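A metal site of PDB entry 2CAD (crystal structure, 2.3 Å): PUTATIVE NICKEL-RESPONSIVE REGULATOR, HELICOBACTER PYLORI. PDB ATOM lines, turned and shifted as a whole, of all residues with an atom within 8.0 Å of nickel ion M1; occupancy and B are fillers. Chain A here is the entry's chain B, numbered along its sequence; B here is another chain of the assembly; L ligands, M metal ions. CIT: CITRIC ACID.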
ATOM      1  N   ASP A  73      19.005   2.745 -30.317  1.00  0.00           N
ATOM      2  CA  ASP A  73      18.438   1.579 -31.022  1.00  0.00           C
ATOM      3  C   ASP A  73      19.566   0.564 -31.251  1.00  0.00           C
ATOM      4  O   ASP A  73      20.514   0.809 -31.989  1.00  0.00           O
ATOM      5  CB  ASP A  73      17.867   2.058 -32.382  1.00  0.00           C
ATOM      6  CG  ASP A  73      17.045   0.976 -33.121  1.00  0.00           C
ATOM      7  OD1 ASP A  73      16.808  -0.153 -32.627  1.00  0.00           O
ATOM      8  OD2 ASP A  73      16.611   1.306 -34.235  1.00  0.00           O
ATOM      9  N   HIS A  74      19.488  -0.589 -30.584  1.00  0.00           N
ATOM     10  CA  HIS A  74      20.555  -1.589 -30.712  1.00  0.00           C
ATOM     11  C   HIS A  74      20.508  -2.296 -32.071  1.00  0.00           C
ATOM     12  O   HIS A  74      21.470  -2.979 -32.444  1.00  0.00           O
ATOM     13  CB  HIS A  74      20.503  -2.605 -29.590  1.00  0.00           C
ATOM     14  CG  HIS A  74      19.520  -3.711 -29.813  1.00  0.00           C
ATOM     15  ND1 HIS A  74      19.916  -4.957 -30.270  1.00  0.00           N
ATOM     16  CD2 HIS A  74      18.190  -3.779 -29.633  1.00  0.00           C
ATOM     17  CE1 HIS A  74      18.854  -5.742 -30.354  1.00  0.00           C
ATOM     18  NE2 HIS A  74      17.798  -5.055 -29.978  1.00  0.00           N
ATOM     19  N   HIS A  75      19.404  -2.127 -32.796  1.00  0.00           N
ATOM     20  CA  HIS A  75      19.329  -2.567 -34.210  1.00  0.00           C
ATOM     21  C   HIS A  75      20.202  -1.797 -35.185  1.00  0.00           C
ATOM     22  O   HIS A  75      20.525  -2.341 -36.218  1.00  0.00           O
ATOM     23  CB  HIS A  75      17.904  -2.574 -34.713  1.00  0.00           C
ATOM     24  CG  HIS A  75      17.053  -3.569 -34.005  1.00  0.00           C
ATOM     25  ND1 HIS A  75      16.919  -4.870 -34.447  1.00  0.00           N
ATOM     26  CD2 HIS A  75      16.338  -3.486 -32.852  1.00  0.00           C
ATOM     27  CE1 HIS A  75      16.123  -5.524 -33.625  1.00  0.00           C
ATOM     28  NE2 HIS A  75      15.761  -4.714 -32.647  1.00  0.00           N
ATOM     29  N   ASP A 103      13.304  -2.010 -24.395  1.00  0.00           N
ATOM     30  CA  ASP A 103      12.370  -2.738 -25.258  1.00  0.00           C
ATOM     31  C   ASP A 103      13.113  -3.216 -26.508  1.00  0.00           C
ATOM     32  O   ASP A 103      14.347  -3.330 -26.501  1.00  0.00           O
ATOM     33  CB  ASP A 103      11.125  -1.893 -25.593  1.00  0.00           C
ATOM     34  CG  ASP A 103      11.441  -0.631 -26.369  1.00  0.00           C
ATOM     35  OD1 ASP A 103      12.123  -0.683 -27.414  1.00  0.00           O
ATOM     36  OD2 ASP A 103      11.006   0.447 -25.923  1.00  0.00           O
ATOM     37  N   GLU A 104      12.362  -3.469 -27.587  1.00  0.00           N
ATOM     38  CA  GLU A 104      12.877  -4.210 -28.742  1.00  0.00           C
ATOM     39  C   GLU A 104      13.936  -3.422 -29.450  1.00  0.00           C
ATOM     40  O   GLU A 104      14.880  -3.978 -30.001  1.00  0.00           O
ATOM     41  CB  GLU A 104      11.755  -4.573 -29.734  1.00  0.00           C
ATOM     42  CG  GLU A 104      10.583  -5.393 -29.125  1.00  0.00           C
ATOM     43  CD  GLU A 104       9.627  -4.541 -28.281  1.00  0.00           C
ATOM     44  OE1 GLU A 104       9.201  -3.471 -28.763  1.00  0.00           O
ATOM     45  OE2 GLU A 104       9.313  -4.938 -27.132  1.00  0.00           O
ATOM     46  N   HIS A 105      13.792  -2.100 -29.438  1.00  0.00           N
ATOM     47  CA  HIS A 105      14.811  -1.238 -29.988  1.00  0.00           C
ATOM     48  C   HIS A 105      15.701  -0.576 -28.917  1.00  0.00           C
ATOM     49  O   HIS A 105      16.944  -0.772 -28.908  1.00  0.00           O
ATOM     50  CB  HIS A 105      14.140  -0.230 -30.916  1.00  0.00           C
ATOM     51  CG  HIS A 105      13.758  -0.829 -32.228  1.00  0.00           C
ATOM     52  ND1 HIS A 105      14.605  -0.815 -33.316  1.00  0.00           N
ATOM     53  CD2 HIS A 105      12.676  -1.541 -32.596  1.00  0.00           C
ATOM     54  CE1 HIS A 105      14.045  -1.464 -34.315  1.00  0.00           C
ATOM     55  NE2 HIS A 105      12.873  -1.915 -33.910  1.00  0.00           N
ATOM     56  N   ASN A 106      15.052   0.122 -27.989  1.00  0.00           N
ATOM     57  CA  ASN A 106      15.694   1.061 -27.051  1.00  0.00           C
ATOM     58  C   ASN A 106      16.515   0.399 -25.959  1.00  0.00           C
ATOM     59  O   ASN A 106      16.011  -0.450 -25.239  1.00  0.00           O
ATOM     60  CB  ASN A 106      14.655   1.967 -26.377  1.00  0.00           C
ATOM     61  CG  ASN A 106      13.806   2.727 -27.366  1.00  0.00           C
ATOM     62  OD1 ASN A 106      14.308   3.585 -28.085  1.00  0.00           O
ATOM     63  ND2 ASN A 106      12.524   2.394 -27.428  1.00  0.00           N
ATOM     64  N   CYS A 107      17.774   0.819 -25.890  1.00  0.00           N
ATOM     65  CA  CYS A 107      18.707   0.593 -24.812  1.00  0.00           C
ATOM     66  C   CYS A 107      18.993   1.956 -24.158  1.00  0.00           C
ATOM     67  O   CYS A 107      19.144   2.953 -24.843  1.00  0.00           O
ATOM     68  CB  CYS A 107      20.029   0.069 -25.365  1.00  0.00           C
ATOM     69  SG  CYS A 107      19.902  -1.528 -26.214  1.00  0.00           S
ATOM     70  N   ILE B  84      24.854  -7.636 -26.654  1.00  0.00           N
ATOM     71  CA  ILE B  84      23.600  -6.863 -26.501  1.00  0.00           C
ATOM     72  C   ILE B  84      22.500  -7.485 -27.334  1.00  0.00           C
ATOM     73  O   ILE B  84      21.395  -7.713 -26.842  1.00  0.00           O
ATOM     74  CB  ILE B  84      23.816  -5.381 -26.885  1.00  0.00           C
ATOM     75  CG1 ILE B  84      24.691  -4.702 -25.812  1.00  0.00           C
ATOM     76  CG2 ILE B  84      22.481  -4.652 -27.038  1.00  0.00           C
ATOM     77  CD1 ILE B  84      25.318  -3.408 -26.266  1.00  0.00           C
ATOM     78  N   ASP B  85      22.801  -7.766 -28.597  1.00  0.00           N
ATOM     79  CA  ASP B  85      21.836  -8.464 -29.446  1.00  0.00           C
ATOM     80  C   ASP B  85      21.347  -9.773 -28.830  1.00  0.00           C
ATOM     81  O   ASP B  85      20.127 -10.036 -28.788  1.00  0.00           O
ATOM     82  CB  ASP B  85      22.412  -8.728 -30.837  1.00  0.00           C
ATOM     83  CG  ASP B  85      22.547  -7.462 -31.668  1.00  0.00           C
ATOM     84  OD1 ASP B  85      21.980  -6.392 -31.307  1.00  0.00           O
ATOM     85  OD2 ASP B  85      23.257  -7.524 -32.672  1.00  0.00           O
ATOM     86  N   GLN B  87      21.365 -10.718 -25.689  1.00  0.00           N
ATOM     87  CA  GLN B  87      20.583 -10.387 -24.496  1.00  0.00           C
ATOM     88  C   GLN B  87      19.202  -9.932 -24.870  1.00  0.00           C
ATOM     89  O   GLN B  87      18.212 -10.366 -24.250  1.00  0.00           O
ATOM     90  CB  GLN B  87      21.313  -9.315 -23.674  1.00  0.00           C
ATOM     91  CG  GLN B  87      22.526  -9.876 -22.958  1.00  0.00           C
ATOM     92  CD  GLN B  87      23.341  -8.816 -22.276  1.00  0.00           C
ATOM     93  OE1 GLN B  87      22.814  -8.039 -21.464  1.00  0.00           O
ATOM     94  NE2 GLN B  87      24.653  -8.783 -22.568  1.00  0.00           N
ATOM     95  N   HIS B  88      19.121  -9.041 -25.867  1.00  0.00           N
ATOM     96  CA  HIS B  88      17.829  -8.616 -26.446  1.00  0.00           C
ATOM     97  C   HIS B  88      17.037  -9.769 -27.054  1.00  0.00           C
ATOM     98  O   HIS B  88      15.833  -9.896 -26.774  1.00  0.00           O
ATOM     99  CB  HIS B  88      18.013  -7.503 -27.493  1.00  0.00           C
ATOM    100  CG  HIS B  88      18.106  -6.130 -26.894  1.00  0.00           C
ATOM    101  ND1 HIS B  88      17.070  -5.219 -26.908  1.00  0.00           N
ATOM    102  CD2 HIS B  88      19.128  -5.515 -26.234  1.00  0.00           C
ATOM    103  CE1 HIS B  88      17.438  -4.121 -26.296  1.00  0.00           C
ATOM    104  NE2 HIS B  88      18.676  -4.276 -25.876  1.00  0.00           N
ATOM    105  N   ALA B  89      17.695 -10.616 -27.861  1.00  0.00           N
ATOM    106  CA  ALA B  89      16.991 -11.770 -28.504  1.00  0.00           C
ATOM    107  C   ALA B  89      16.566 -12.869 -27.535  1.00  0.00           C
ATOM    108  O   ALA B  89      15.626 -13.610 -27.826  1.00  0.00           O
ATOM    109  CB  ALA B  89      17.865 -12.377 -29.566  1.00  0.00           C
HETATM  110  C1  CIT L   1      14.461  -7.249 -28.128  1.00  0.00           C
HETATM  111  O1  CIT L   1      14.209  -7.234 -26.891  1.00  0.00           O
HETATM  112  O2  CIT L   1      15.151  -6.302 -28.564  1.00  0.00           O
HETATM  113  C2  CIT L   1      13.954  -8.366 -29.044  1.00  0.00           C
HETATM  114  C3  CIT L   1      14.266  -8.185 -30.541  1.00  0.00           C
HETATM  115  O7  CIT L   1      14.026  -6.802 -30.904  1.00  0.00           O
HETATM  116  C4  CIT L   1      13.345  -9.047 -31.403  1.00  0.00           C
HETATM  117  C5  CIT L   1      13.585  -8.948 -32.904  1.00  0.00           C
HETATM  118  O3  CIT L   1      14.613  -8.426 -33.438  1.00  0.00           O
HETATM  119  O4  CIT L   1      12.695  -9.426 -33.634  1.00  0.00           O
HETATM  120  C6  CIT L   1      15.705  -8.595 -30.872  1.00  0.00           C
HETATM  121  O5  CIT L   1      16.528  -7.772 -31.294  1.00  0.00           O
HETATM  122  O6  CIT L   1      16.074  -9.791 -30.785  1.00  0.00           O
HETATM  123 NI    NI M   1      15.858  -5.606 -30.588  1.00  0.00          NI
HETATM  124 NI    NI M   2      19.979  -3.243 -24.706  1.00  0.00          NI
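A ring nitrogen (NE2) of His 74 lies close to a ring nitrogen (ND1) of His 88 of chain B.
N of His 74 is in hydrogen-bond range of O of His 105, at 3.1 Å.
ND1 of His 74 is in hydrogen-bond range of OD1 of Asp 85 of chain B.
The backbone NH (N) of His 75 sits close to the side-chain carboxylate (OD1) of Asp 73 (3.3 Å).
A ring nitrogen (ND1) of His 88 of chain B lies close to the backbone carbonyl oxygen of Asp 103 (3.3 Å).
Residues that only touch nickel ion M1: His 88 of chain B (3.9 Å).
Four residues have an atom within 4 Å of nickel ion M1: His 74, His 75, Glu 104 and His 88 of chain B.
Nickel ion M1 is bound by the backbone carbonyl oxygen of Glu 104, a ring nitrogen (NE2) of His 74, an oxygen (O7) of the ligand, a ring nitrogen (NE2) of His 75, an oxygen (O2) of the ligand and an oxygen (O5) of the ligand.
Nickel ion M1 has six donor atoms within binding distance.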
